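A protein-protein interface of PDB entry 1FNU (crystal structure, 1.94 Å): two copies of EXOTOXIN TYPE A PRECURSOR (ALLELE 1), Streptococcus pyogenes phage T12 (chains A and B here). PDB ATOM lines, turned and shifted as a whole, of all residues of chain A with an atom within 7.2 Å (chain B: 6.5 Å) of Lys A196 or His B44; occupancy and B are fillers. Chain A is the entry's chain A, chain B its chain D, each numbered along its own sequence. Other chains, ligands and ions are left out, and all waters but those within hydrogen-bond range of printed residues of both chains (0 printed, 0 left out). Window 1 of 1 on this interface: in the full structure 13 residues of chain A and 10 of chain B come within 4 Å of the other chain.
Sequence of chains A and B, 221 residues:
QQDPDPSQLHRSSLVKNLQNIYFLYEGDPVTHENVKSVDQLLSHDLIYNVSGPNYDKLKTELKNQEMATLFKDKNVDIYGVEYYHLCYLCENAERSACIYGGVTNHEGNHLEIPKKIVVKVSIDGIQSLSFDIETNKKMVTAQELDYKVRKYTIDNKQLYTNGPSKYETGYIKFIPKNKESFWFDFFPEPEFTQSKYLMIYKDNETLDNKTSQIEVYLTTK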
ATOM      1  N   HIS A  10       8.090 -35.362 -18.439  1.00  0.00           N
ATOM      2  CA  HIS A  10       6.890 -34.658 -18.926  1.00  0.00           C
ATOM      3  C   HIS A  10       6.250 -35.517 -20.018  1.00  0.00           C
ATOM      4  O   HIS A  10       6.919 -35.957 -20.947  1.00  0.00           O
ATOM      5  CB  HIS A  10       7.288 -33.280 -19.510  1.00  0.00           C
ATOM      6  CG  HIS A  10       7.858 -32.322 -18.509  1.00  0.00           C
ATOM      7  ND1 HIS A  10       8.602 -31.219 -18.880  1.00  0.00           N
ATOM      8  CD2 HIS A  10       7.678 -32.209 -17.169  1.00  0.00           C
ATOM      9  CE1 HIS A  10       8.855 -30.467 -17.816  1.00  0.00           C
ATOM     10  NE2 HIS A  10       8.304 -31.043 -16.764  1.00  0.00           N
ATOM     11  N   TYR A  83      14.201 -18.488 -30.766  1.00  0.00           N
ATOM     12  CA  TYR A  83      12.794 -18.127 -30.574  1.00  0.00           C
ATOM     13  C   TYR A  83      12.636 -16.629 -30.792  1.00  0.00           C
ATOM     14  O   TYR A  83      13.577 -15.816 -30.629  1.00  0.00           O
ATOM     15  CB  TYR A  83      12.246 -18.460 -29.172  1.00  0.00           C
ATOM     16  CG  TYR A  83      12.816 -17.642 -28.041  1.00  0.00           C
ATOM     17  CD1 TYR A  83      14.030 -18.007 -27.451  1.00  0.00           C
ATOM     18  CD2 TYR A  83      12.159 -16.527 -27.548  1.00  0.00           C
ATOM     19  CE1 TYR A  83      14.598 -17.264 -26.365  1.00  0.00           C
ATOM     20  CE2 TYR A  83      12.724 -15.765 -26.421  1.00  0.00           C
ATOM     21  CZ  TYR A  83      13.946 -16.169 -25.866  1.00  0.00           C
ATOM     22  OH  TYR A  83      14.461 -15.465 -24.807  1.00  0.00           O
ATOM     23  N   LEU A  86       8.337 -13.324 -27.317  1.00  0.00           N
ATOM     24  CA  LEU A  86       8.891 -12.878 -26.019  1.00  0.00           C
ATOM     25  C   LEU A  86      10.456 -12.736 -26.021  1.00  0.00           C
ATOM     26  O   LEU A  86      11.122 -12.821 -24.985  1.00  0.00           O
ATOM     27  CB  LEU A  86       8.513 -13.809 -24.866  1.00  0.00           C
ATOM     28  CG  LEU A  86       7.008 -14.087 -24.809  1.00  0.00           C
ATOM     29  CD1 LEU A  86       6.659 -15.049 -23.649  1.00  0.00           C
ATOM     30  CD2 LEU A  86       6.286 -12.646 -24.687  1.00  0.00           C
ATOM     31  N   TYR A 100      19.522 -19.232 -25.786  1.00  0.00           N
ATOM     32  CA  TYR A 100      20.071 -19.392 -24.466  1.00  0.00           C
ATOM     33  C   TYR A 100      21.369 -20.164 -24.742  1.00  0.00           C
ATOM     34  O   TYR A 100      21.435 -21.023 -25.653  1.00  0.00           O
ATOM     35  CB  TYR A 100      19.157 -20.177 -23.557  1.00  0.00           C
ATOM     36  CG  TYR A 100      17.975 -19.367 -23.058  1.00  0.00           C
ATOM     37  CD1 TYR A 100      18.058 -18.543 -21.918  1.00  0.00           C
ATOM     38  CD2 TYR A 100      16.765 -19.432 -23.744  1.00  0.00           C
ATOM     39  CE1 TYR A 100      16.934 -17.805 -21.479  1.00  0.00           C
ATOM     40  CE2 TYR A 100      15.660 -18.722 -23.343  1.00  0.00           C
ATOM     41  CZ  TYR A 100      15.734 -17.931 -22.243  1.00  0.00           C
ATOM     42  OH  TYR A 100      14.616 -17.306 -21.885  1.00  0.00           O
ATOM     43  N   PRO A 188       8.024 -30.233 -22.803  1.00  0.00           N
ATOM     44  CA  PRO A 188       7.752 -29.128 -21.898  1.00  0.00           C
ATOM     45  C   PRO A 188       6.620 -29.467 -20.921  1.00  0.00           C
ATOM     46  O   PRO A 188       5.962 -30.502 -21.073  1.00  0.00           O
ATOM     47  CB  PRO A 188       7.279 -28.028 -22.872  1.00  0.00           C
ATOM     48  CG  PRO A 188       6.409 -28.805 -23.801  1.00  0.00           C
ATOM     49  CD  PRO A 188       7.447 -29.934 -24.139  1.00  0.00           C
ATOM     50  N   GLU A 189       6.367 -28.562 -19.953  1.00  0.00           N
ATOM     51  CA  GLU A 189       5.205 -28.697 -19.073  1.00  0.00           C
ATOM     52  C   GLU A 189       3.957 -28.476 -20.012  1.00  0.00           C
ATOM     53  O   GLU A 189       4.093 -27.981 -21.161  1.00  0.00           O
ATOM     54  CB  GLU A 189       5.215 -27.698 -17.904  1.00  0.00           C
ATOM     55  CG  GLU A 189       5.392 -26.284 -18.269  1.00  0.00           C
ATOM     56  CD  GLU A 189       5.206 -25.366 -17.084  1.00  0.00           C
ATOM     57  OE1 GLU A 189       5.319 -25.813 -15.900  1.00  0.00           O
ATOM     58  OE2 GLU A 189       4.929 -24.179 -17.365  1.00  0.00           O
ATOM     59  N   PRO A 190       2.730 -28.814 -19.529  1.00  0.00           N
ATOM     60  CA  PRO A 190       1.524 -28.683 -20.348  1.00  0.00           C
ATOM     61  C   PRO A 190       1.251 -27.349 -21.025  1.00  0.00           C
ATOM     62  O   PRO A 190       1.027 -27.313 -22.219  1.00  0.00           O
ATOM     63  CB  PRO A 190       0.439 -29.185 -19.380  1.00  0.00           C
ATOM     64  CG  PRO A 190       1.172 -30.183 -18.548  1.00  0.00           C
ATOM     65  CD  PRO A 190       2.351 -29.281 -18.190  1.00  0.00           C
ATOM     66  N   GLU A 191       1.257 -26.259 -20.267  1.00  0.00           N
ATOM     67  CA  GLU A 191       1.085 -24.933 -20.831  1.00  0.00           C
ATOM     68  C   GLU A 191       2.465 -24.283 -20.613  1.00  0.00           C
ATOM     69  O   GLU A 191       2.954 -24.089 -19.465  1.00  0.00           O
ATOM     70  CB  GLU A 191      -0.036 -24.198 -20.110  1.00  0.00           C
ATOM     71  CG  GLU A 191      -1.342 -24.953 -20.274  1.00  0.00           C
ATOM     72  CD  GLU A 191      -1.927 -25.342 -18.897  1.00  0.00           C
ATOM     73  OE1 GLU A 191      -2.464 -24.409 -18.138  1.00  0.00           O
ATOM     74  OE2 GLU A 191      -1.793 -26.591 -18.546  1.00  0.00           O
ATOM     75  N   PHE A 192       3.087 -23.955 -21.737  1.00  0.00           N
ATOM     76  CA  PHE A 192       4.469 -23.449 -21.701  1.00  0.00           C
ATOM     77  C   PHE A 192       4.724 -22.383 -22.721  1.00  0.00           C
ATOM     78  O   PHE A 192       3.825 -22.026 -23.518  1.00  0.00           O
ATOM     79  CB  PHE A 192       5.456 -24.626 -22.015  1.00  0.00           C
ATOM     80  CG  PHE A 192       5.383 -25.113 -23.445  1.00  0.00           C
ATOM     81  CD1 PHE A 192       4.261 -25.815 -23.902  1.00  0.00           C
ATOM     82  CD2 PHE A 192       6.388 -24.726 -24.411  1.00  0.00           C
ATOM     83  CE1 PHE A 192       4.087 -26.132 -25.243  1.00  0.00           C
ATOM     84  CE2 PHE A 192       6.226 -25.032 -25.790  1.00  0.00           C
ATOM     85  CZ  PHE A 192       5.045 -25.755 -26.236  1.00  0.00           C
ATOM     86  N   THR A 193       5.932 -21.825 -22.679  1.00  0.00           N
ATOM     87  CA  THR A 193       6.331 -20.921 -23.752  1.00  0.00           C
ATOM     88  C   THR A 193       7.699 -21.417 -24.160  1.00  0.00           C
ATOM     89  O   THR A 193       8.483 -22.011 -23.345  1.00  0.00           O
ATOM     90  CB  THR A 193       6.511 -19.394 -23.321  1.00  0.00           C
ATOM     91  OG1 THR A 193       7.489 -19.328 -22.284  1.00  0.00           O
ATOM     92  CG2 THR A 193       5.220 -18.782 -22.904  1.00  0.00           C
ATOM     93  N   GLN A 194       8.011 -21.155 -25.413  1.00  0.00           N
ATOM     94  CA  GLN A 194       9.304 -21.542 -25.983  1.00  0.00           C
ATOM     95  C   GLN A 194      10.494 -20.921 -25.173  1.00  0.00           C
ATOM     96  O   GLN A 194      11.551 -21.575 -24.899  1.00  0.00           O
ATOM     97  CB  GLN A 194       9.332 -21.085 -27.451  1.00  0.00           C
ATOM     98  CG  GLN A 194       8.510 -21.926 -28.392  1.00  0.00           C
ATOM     99  CD  GLN A 194       8.349 -21.229 -29.760  1.00  0.00           C
ATOM    100  OE1 GLN A 194       8.179 -21.859 -30.836  1.00  0.00           O
ATOM    101  NE2 GLN A 194       8.396 -19.903 -29.720  1.00  0.00           N
ATOM    102  N   SER A 195      10.287 -19.679 -24.761  1.00  0.00           N
ATOM    103  CA  SER A 195      11.282 -18.925 -24.013  1.00  0.00           C
ATOM    104  C   SER A 195      11.644 -19.629 -22.688  1.00  0.00           C
ATOM    105  O   SER A 195      12.813 -19.672 -22.315  1.00  0.00           O
ATOM    106  CB  SER A 195      10.746 -17.519 -23.697  1.00  0.00           C
ATOM    107  OG  SER A 195      11.692 -16.798 -22.932  1.00  0.00           O
ATOM    108  N   LYS A 196      10.628 -20.082 -21.962  1.00  0.00           N
ATOM    109  CA  LYS A 196      10.851 -20.766 -20.700  1.00  0.00           C
ATOM    110  C   LYS A 196      11.499 -22.178 -20.866  1.00  0.00           C
ATOM    111  O   LYS A 196      12.461 -22.504 -20.171  1.00  0.00           O
ATOM    112  CB  LYS A 196       9.545 -20.864 -19.893  1.00  0.00           C
ATOM    113  CG  LYS A 196       8.745 -22.139 -20.291  1.00  0.00           C
ATOM    114  CD  LYS A 196       7.471 -22.659 -19.415  1.00  0.00           C
ATOM    115  CE  LYS A 196       7.753 -22.791 -17.855  1.00  0.00           C
ATOM    116  NZ  LYS A 196       8.896 -23.784 -17.368  1.00  0.00           N
ATOM    117  N   TYR A 197      11.028 -22.929 -21.866  1.00  0.00           N
ATOM    118  CA  TYR A 197      11.472 -24.260 -22.206  1.00  0.00           C
ATOM    119  C   TYR A 197      12.949 -24.236 -22.596  1.00  0.00           C
ATOM    120  O   TYR A 197      13.725 -25.117 -22.172  1.00  0.00           O
ATOM    121  CB  TYR A 197      10.743 -24.826 -23.443  1.00  0.00           C
ATOM    122  CG  TYR A 197      11.223 -26.222 -23.811  1.00  0.00           C
ATOM    123  CD1 TYR A 197      10.973 -27.302 -22.957  1.00  0.00           C
ATOM    124  CD2 TYR A 197      12.091 -26.420 -24.901  1.00  0.00           C
ATOM    125  CE1 TYR A 197      11.578 -28.515 -23.141  1.00  0.00           C
ATOM    126  CE2 TYR A 197      12.692 -27.629 -25.091  1.00  0.00           C
ATOM    127  CZ  TYR A 197      12.441 -28.674 -24.199  1.00  0.00           C
ATOM    128  OH  TYR A 197      13.065 -29.895 -24.386  1.00  0.00           O
ATOM    129  N   LEU A 198      13.361 -23.230 -23.380  1.00  0.00           N
ATOM    130  CA  LEU A 198      14.730 -23.222 -23.895  1.00  0.00           C
ATOM    131  C   LEU A 198      15.849 -22.915 -22.871  1.00  0.00           C
ATOM    132  O   LEU A 198      17.061 -23.032 -23.164  1.00  0.00           O
ATOM    133  CB  LEU A 198      14.770 -22.316 -25.170  1.00  0.00           C
ATOM    134  CG  LEU A 198      14.055 -22.941 -26.421  1.00  0.00           C
ATOM    135  CD1 LEU A 198      13.988 -21.952 -27.562  1.00  0.00           C
ATOM    136  CD2 LEU A 198      14.877 -24.193 -26.905  1.00  0.00           C
ATOM    137  N   MET A 199      15.416 -22.607 -21.658  1.00  0.00           N
ATOM    138  CA  MET A 199      16.304 -22.312 -20.571  1.00  0.00           C
ATOM    139  C   MET A 199      17.060 -23.597 -20.244  1.00  0.00           C
ATOM    140  O   MET A 199      17.993 -23.518 -19.500  1.00  0.00           O
ATOM    141  CB  MET A 199      15.542 -21.723 -19.370  1.00  0.00           C
ATOM    142  CG  MET A 199      15.059 -20.267 -19.637  1.00  0.00           C
ATOM    143  SD  MET A 199      13.982 -19.563 -18.307  1.00  0.00           S
ATOM    144  CE  MET A 199      15.050 -19.315 -17.067  1.00  0.00           C
ATOM    145  N   ILE A 200      16.713 -24.758 -20.810  1.00  0.00           N
ATOM    146  CA  ILE A 200      17.607 -25.912 -20.556  1.00  0.00           C
ATOM    147  C   ILE A 200      19.024 -25.657 -21.136  1.00  0.00           C
ATOM    148  O   ILE A 200      19.984 -26.352 -20.779  1.00  0.00           O
ATOM    149  CB  ILE A 200      17.045 -27.238 -21.186  1.00  0.00           C
ATOM    150  CG1 ILE A 200      16.745 -26.978 -22.664  1.00  0.00           C
ATOM    151  CG2 ILE A 200      15.831 -27.744 -20.294  1.00  0.00           C
ATOM    152  CD1 ILE A 200      16.533 -28.186 -23.543  1.00  0.00           C
ATOM    153  N   GLN B  40      -4.829 -20.077 -14.396  1.00  0.00           N
ATOM    154  CA  GLN B  40      -3.362 -20.052 -14.335  1.00  0.00           C
ATOM    155  C   GLN B  40      -2.982 -19.764 -15.794  1.00  0.00           C
ATOM    156  O   GLN B  40      -3.808 -19.946 -16.682  1.00  0.00           O
ATOM    157  CB  GLN B  40      -2.764 -21.377 -13.793  1.00  0.00           C
ATOM    158  CG  GLN B  40      -2.693 -22.484 -14.757  1.00  0.00           C
ATOM    159  CD  GLN B  40      -2.229 -23.832 -14.129  1.00  0.00           C
ATOM    160  OE1 GLN B  40      -1.464 -23.874 -13.167  1.00  0.00           O
ATOM    161  NE2 GLN B  40      -2.661 -24.923 -14.724  1.00  0.00           N
ATOM    162  N   LEU B  41      -1.783 -19.264 -16.050  1.00  0.00           N
ATOM    163  CA  LEU B  41      -1.424 -18.967 -17.431  1.00  0.00           C
ATOM    164  C   LEU B  41      -0.483 -20.074 -17.930  1.00  0.00           C
ATOM    165  O   LEU B  41      -0.777 -20.726 -18.924  1.00  0.00           O
ATOM    166  CB  LEU B  41      -0.745 -17.618 -17.512  1.00  0.00           C
ATOM    167  CG  LEU B  41      -0.225 -17.251 -18.916  1.00  0.00           C
ATOM    168  CD1 LEU B  41      -1.368 -17.060 -19.935  1.00  0.00           C
ATOM    169  CD2 LEU B  41       0.642 -16.020 -18.716  1.00  0.00           C
ATOM    170  N   LEU B  42       0.651 -20.251 -17.287  1.00  0.00           N
ATOM    171  CA  LEU B  42       1.520 -21.377 -17.616  1.00  0.00           C
ATOM    172  C   LEU B  42       1.210 -22.462 -16.559  1.00  0.00           C
ATOM    173  O   LEU B  42       0.458 -22.212 -15.571  1.00  0.00           O
ATOM    174  CB  LEU B  42       3.007 -20.946 -17.566  1.00  0.00           C
ATOM    175  CG  LEU B  42       3.207 -19.820 -18.602  1.00  0.00           C
ATOM    176  CD1 LEU B  42       4.714 -19.379 -18.742  1.00  0.00           C
ATOM    177  CD2 LEU B  42       2.652 -20.315 -19.959  1.00  0.00           C
ATOM    178  N   SER B  43       1.759 -23.668 -16.718  1.00  0.00           N
ATOM    179  CA  SER B  43       1.388 -24.694 -15.740  1.00  0.00           C
ATOM    180  C   SER B  43       2.022 -24.484 -14.391  1.00  0.00           C
ATOM    181  O   SER B  43       1.662 -25.185 -13.409  1.00  0.00           O
ATOM    182  CB  SER B  43       1.748 -26.110 -16.211  1.00  0.00           C
ATOM    183  OG  SER B  43       1.179 -26.374 -17.461  1.00  0.00           O
ATOM    184  N   HIS B  44       2.958 -23.550 -14.309  1.00  0.00           N
ATOM    185  CA  HIS B  44       3.631 -23.349 -13.039  1.00  0.00           C
ATOM    186  C   HIS B  44       3.305 -22.080 -12.201  1.00  0.00           C
ATOM    187  O   HIS B  44       4.021 -21.783 -11.216  1.00  0.00           O
ATOM    188  CB  HIS B  44       5.094 -23.359 -13.233  1.00  0.00           C
ATOM    189  CG  HIS B  44       5.568 -22.149 -13.962  1.00  0.00           C
ATOM    190  ND1 HIS B  44       5.658 -22.099 -15.342  1.00  0.00           N
ATOM    191  CD2 HIS B  44       6.054 -20.972 -13.507  1.00  0.00           C
ATOM    192  CE1 HIS B  44       6.200 -20.948 -15.695  1.00  0.00           C
ATOM    193  NE2 HIS B  44       6.449 -20.243 -14.601  1.00  0.00           N
ATOM    194  N   ASP B  45       2.227 -21.395 -12.577  1.00  0.00           N
ATOM    195  CA  ASP B  45       1.713 -20.211 -11.873  1.00  0.00           C
ATOM    196  C   ASP B  45       0.238 -20.500 -11.523  1.00  0.00           C
ATOM    197  O   ASP B  45      -0.294 -21.534 -11.903  1.00  0.00           O
ATOM    198  CB  ASP B  45       1.793 -18.914 -12.747  1.00  0.00           C
ATOM    199  CG  ASP B  45       0.937 -18.971 -13.997  1.00  0.00           C
ATOM    200  OD1 ASP B  45      -0.285 -19.088 -13.922  1.00  0.00           O
ATOM    201  OD2 ASP B  45       1.475 -18.897 -15.116  1.00  0.00           O
ATOM    202  N   LEU B  46      -0.374 -19.580 -10.769  1.00  0.00           N
ATOM    203  CA  LEU B  46      -1.770 -19.654 -10.368  1.00  0.00           C
ATOM    204  C   LEU B  46      -2.180 -18.187 -10.388  1.00  0.00           C
ATOM    205  O   LEU B  46      -1.384 -17.348 -10.036  1.00  0.00           O
ATOM    206  CB  LEU B  46      -1.894 -20.168  -8.928  1.00  0.00           C
ATOM    207  CG  LEU B  46      -1.537 -21.628  -8.680  1.00  0.00           C
ATOM    208  CD1 LEU B  46      -1.712 -21.996  -7.200  1.00  0.00           C
ATOM    209  CD2 LEU B  46      -2.485 -22.459  -9.535  1.00  0.00           C
ATOM    210  N   LYS B  59      -1.016 -12.613 -10.226  1.00  0.00           N
ATOM    211  CA  LYS B  59      -0.420 -13.884 -10.603  1.00  0.00           C
ATOM    212  C   LYS B  59       0.850 -14.273  -9.779  1.00  0.00           C
ATOM    213  O   LYS B  59       1.754 -13.456  -9.550  1.00  0.00           O
ATOM    214  CB  LYS B  59      -0.006 -13.911 -12.060  1.00  0.00           C
ATOM    215  CG  LYS B  59       0.648 -15.291 -12.437  1.00  0.00           C
ATOM    216  CD  LYS B  59       1.155 -15.337 -13.890  1.00  0.00           C
ATOM    217  CE  LYS B  59       2.565 -14.586 -13.937  1.00  0.00           C
ATOM    218  NZ  LYS B  59       3.285 -14.714 -15.223  1.00  0.00           N
ATOM    219  N   THR B  60       0.918 -15.536  -9.352  1.00  0.00           N
ATOM    220  CA  THR B  60       2.122 -15.980  -8.669  1.00  0.00           C
ATOM    221  C   THR B  60       2.688 -17.171  -9.417  1.00  0.00           C
ATOM    222  O   THR B  60       1.906 -18.095  -9.745  1.00  0.00           O
ATOM    223  CB  THR B  60       1.915 -16.419  -7.224  1.00  0.00           C
ATOM    224  OG1 THR B  60       3.184 -16.662  -6.658  1.00  0.00           O
ATOM    225  CG2 THR B  60       1.151 -17.677  -7.096  1.00  0.00           C
ATOM    226  N   GLU B  61       4.006 -17.110  -9.676  1.00  0.00           N
ATOM    227  CA  GLU B  61       4.783 -18.159 -10.344  1.00  0.00           C
ATOM    228  C   GLU B  61       5.469 -18.909  -9.261  1.00  0.00           C
ATOM    229  O   GLU B  61       6.315 -18.354  -8.590  1.00  0.00           O
ATOM    230  CB  GLU B  61       5.883 -17.597 -11.268  1.00  0.00           C
ATOM    231  CG  GLU B  61       5.350 -17.033 -12.551  1.00  0.00           C
ATOM    232  CD  GLU B  61       6.445 -16.580 -13.531  1.00  0.00           C
ATOM    233  OE1 GLU B  61       7.272 -17.473 -13.937  1.00  0.00           O
ATOM    234  OE2 GLU B  61       6.407 -15.340 -13.841  1.00  0.00           O
ATOM    235  N   LEU B  62       5.104 -20.179  -9.143  1.00  0.00           N
ATOM    236  CA  LEU B  62       5.646 -21.110  -8.119  1.00  0.00           C
ATOM    237  C   LEU B  62       6.795 -21.944  -8.690  1.00  0.00           C
ATOM    238  O   LEU B  62       7.333 -21.641  -9.756  1.00  0.00           O
ATOM    239  CB  LEU B  62       4.496 -22.044  -7.579  1.00  0.00           C
ATOM    240  CG  LEU B  62       3.385 -21.231  -6.881  1.00  0.00           C
ATOM    241  CD1 LEU B  62       2.026 -21.869  -6.974  1.00  0.00           C
ATOM    242  CD2 LEU B  62       3.853 -20.988  -5.445  1.00  0.00           C
ATOM    243  N   LYS B  63       7.153 -23.032  -7.989  1.00  0.00           N
ATOM    244  CA  LYS B  63       8.312 -23.828  -8.412  1.00  0.00           C
ATOM    245  C   LYS B  63       8.218 -24.647  -9.708  1.00  0.00           C
ATOM    246  O   LYS B  63       9.196 -24.689 -10.474  1.00  0.00           O
ATOM    247  CB  LYS B  63       8.784 -24.692  -7.212  1.00  0.00           C
ATOM    248  CG  LYS B  63      10.141 -25.435  -7.414  1.00  0.00           C
ATOM    249  CD  LYS B  63      10.603 -26.043  -6.025  1.00  0.00           C
ATOM    250  CE  LYS B  63      12.209 -26.276  -5.842  1.00  0.00           C
ATOM    251  NZ  LYS B  63      12.659 -26.283  -4.291  1.00  0.00           N
ATOM    252  N   ASN B  64       7.036 -25.201 -10.000  1.00  0.00           N
ATOM    253  CA  ASN B  64       6.832 -26.040 -11.170  1.00  0.00           C
ATOM    254  C   ASN B  64       5.367 -26.383 -11.249  1.00  0.00           C
ATOM    255  O   ASN B  64       4.553 -25.901 -10.430  1.00  0.00           O
ATOM    256  CB  ASN B  64       7.638 -27.320 -10.989  1.00  0.00           C
ATOM    257  CG  ASN B  64       7.441 -27.914  -9.565  1.00  0.00           C
ATOM    258  OD1 ASN B  64       6.288 -28.138  -9.115  1.00  0.00           O
ATOM    259  ND2 ASN B  64       8.549 -28.141  -8.850  1.00  0.00           N
ATOM    260  N   GLN B  65       5.000 -27.243 -12.196  1.00  0.00           N
ATOM    261  CA  GLN B  65       3.597 -27.627 -12.329  1.00  0.00           C
ATOM    262  C   GLN B  65       3.004 -28.405 -11.065  1.00  0.00           C
ATOM    263  O   GLN B  65       1.809 -28.220 -10.696  1.00  0.00           O
ATOM    264  CB  GLN B  65       3.430 -28.398 -13.633  1.00  0.00           C
ATOM    265  CG  GLN B  65       3.559 -29.906 -13.536  1.00  0.00           C
ATOM    266  CD  GLN B  65       3.620 -30.528 -14.895  1.00  0.00           C
ATOM    267  OE1 GLN B  65       4.700 -30.920 -15.384  1.00  0.00           O
ATOM    268  NE2 GLN B  65       2.485 -30.569 -15.554  1.00  0.00           N
ATOM    269  N   GLU B  66       3.847 -29.223 -10.408  1.00  0.00           N
ATOM    270  CA  GLU B  66       3.441 -29.998  -9.226  1.00  0.00           C
ATOM    271  C   GLU B  66       3.140 -29.100  -8.047  1.00  0.00           C
ATOM    272  O   GLU B  66       2.158 -29.324  -7.332  1.00  0.00           O
ATOM    273  CB  GLU B  66       4.506 -31.016  -8.850  1.00  0.00           C
ATOM    274  CG  GLU B  66       4.845 -31.929 -10.039  1.00  0.00           C
ATOM    275  CD  GLU B  66       6.108 -31.504 -10.877  1.00  0.00           C
ATOM    276  OE1 GLU B  66       6.171 -30.376 -11.490  1.00  0.00           O
ATOM    277  OE2 GLU B  66       7.046 -32.356 -10.910  1.00  0.00           O
ATOM    278  N   MET B  67       3.945 -28.078  -7.807  1.00  0.00           N
ATOM    279  CA  MET B  67       3.562 -27.210  -6.715  1.00  0.00           C
ATOM    280  C   MET B  67       2.246 -26.445  -7.087  1.00  0.00           C
ATOM    281  O   MET B  67       1.281 -26.344  -6.292  1.00  0.00           O
ATOM    282  CB  MET B  67       4.657 -26.234  -6.435  1.00  0.00           C
ATOM    283  CG  MET B  67       4.318 -25.271  -5.327  1.00  0.00           C
ATOM    284  SD  MET B  67       5.794 -24.249  -5.039  1.00  0.00           S
ATOM    285  CE  MET B  67       6.984 -25.430  -4.419  1.00  0.00           C
ATOM    286  N   ALA B  68       2.173 -25.940  -8.307  1.00  0.00           N
ATOM    287  CA  ALA B  68       0.976 -25.216  -8.680  1.00  0.00           C
ATOM    288  C   ALA B  68      -0.263 -26.072  -8.602  1.00  0.00           C
ATOM    289  O   ALA B  68      -1.257 -25.605  -8.062  1.00  0.00           O
ATOM    290  CB  ALA B  68       1.103 -24.602 -10.080  1.00  0.00           C
ATOM    291  N   LYS B 202      10.746 -17.601  -6.090  1.00  0.00           N
ATOM    292  CA  LYS B 202      10.095 -18.641  -6.896  1.00  0.00           C
ATOM    293  C   LYS B 202      10.118 -20.042  -6.257  1.00  0.00           C
ATOM    294  O   LYS B 202       9.202 -20.837  -6.458  1.00  0.00           O
ATOM    295  CB  LYS B 202      10.752 -18.670  -8.280  1.00  0.00           C
ATOM    296  CG  LYS B 202      10.157 -19.669  -9.235  1.00  0.00           C
ATOM    297  CD  LYS B 202      10.816 -19.510 -10.663  1.00  0.00           C
ATOM    298  CE  LYS B 202      10.536 -20.696 -11.654  1.00  0.00           C
ATOM    299  NZ  LYS B 202       9.119 -21.195 -11.818  1.00  0.00           N
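N of Lys A196 lies within hydrogen-bond range of OG1 of Thr A193 (3.2 Å).
O of Leu B42 sits close to OE1 of Gln B40 (3.5 Å).
The side-chain amide oxygen (OE1) of Gln B40 lies close to the backbone carbonyl oxygen (O) of Asp B45 (2.9 Å).
N of Leu B41 sits at hydrogen-bond distance from OD1 of Asp B45, 2.6 Å away.
NE2 of His B44 lies within hydrogen-bond range of OE1 of Glu B61, at 3.0 Å.
The backbone carbonyl oxygen (O) of His B44 sits at hydrogen-bond distance from the backbone NH (N) of Leu B62 (2.8 Å).
Among the printed residues, pairs that only touch across the chains: Pro A190 with Gln B65 (2.9 Å), Pro A190 with Ser B43 (3.2 Å), Lys A196 with His B44 (3.2 Å), Glu A191 with Leu B42 (3.6 Å), His A10 with Gln B65 (3.7 Å), Glu A191 with Leu B41 (3.7 Å), Glu A189 with Leu B42 (3.8 Å) and Glu A189 with Gln B65 (3.9 Å).
No position is printed for both chains.
Of the 12 pairs that touch across the chains among the printed residues, none has its exchanged pair printed and touching as well.
Hydrophobic or aromatic side chains of chain B within 4 Å of the printed part of chain A: Leu B42 and His B44.
Of the 17 printed residues of chain A, 5 touch a printed residue of chain B.
Printed residues of chain A that touch a printed residue of chain B: His A10, Glu A189, Pro A190, Glu A191 and Lys A196.
Hydrophobic or aromatic side chains of chain A within 4 Å of the printed part of chain B: His A10 and Pro A190.
Among the printed residues, 12 pairs touch across the chains.
Among the printed residues, no Asp or Glu carboxylate lies within 4 Å of a Lys or Arg side-chain nitrogen of the other chain.
Lys A196 touches just one residue of chain B: His B44 (3.2 Å).
His B44 touches just these residues of chain A: Glu A189 and Lys A196.
Of the printed residues of chain A, Leu B42 touches Glu A189 and Glu A191.
Of the printed residues of chain B, Pro A190 touches Ser B43 (3.2 Å) and Gln B65 (2.9 Å).
Of the printed residues of chain A, Gln B65 touches His A10, Glu A189 and Pro A190.
Of the printed residues of chain A, Leu B41 touches Glu A191.
Of the printed residues of chain B, His A10 touches Gln B65.
Ser A195 touches none of the printed residues of chain B.
The nearest printed residue of chain A that does not touch Gln B40 is Pro A190 (7.0 Å).
OE2 of Glu A189 sits at hydrogen-bond distance from N of Ser B43 (3.3 Å).
OE2 of Glu A189 sits at hydrogen-bond distance from ND1 of His B44 (3.0 Å).
NE2 of Gln B40 is in hydrogen-bond range of OE1 of Glu A191 (3.5 Å).
OG of Ser B43 is in hydrogen-bond range of N of Glu A191.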
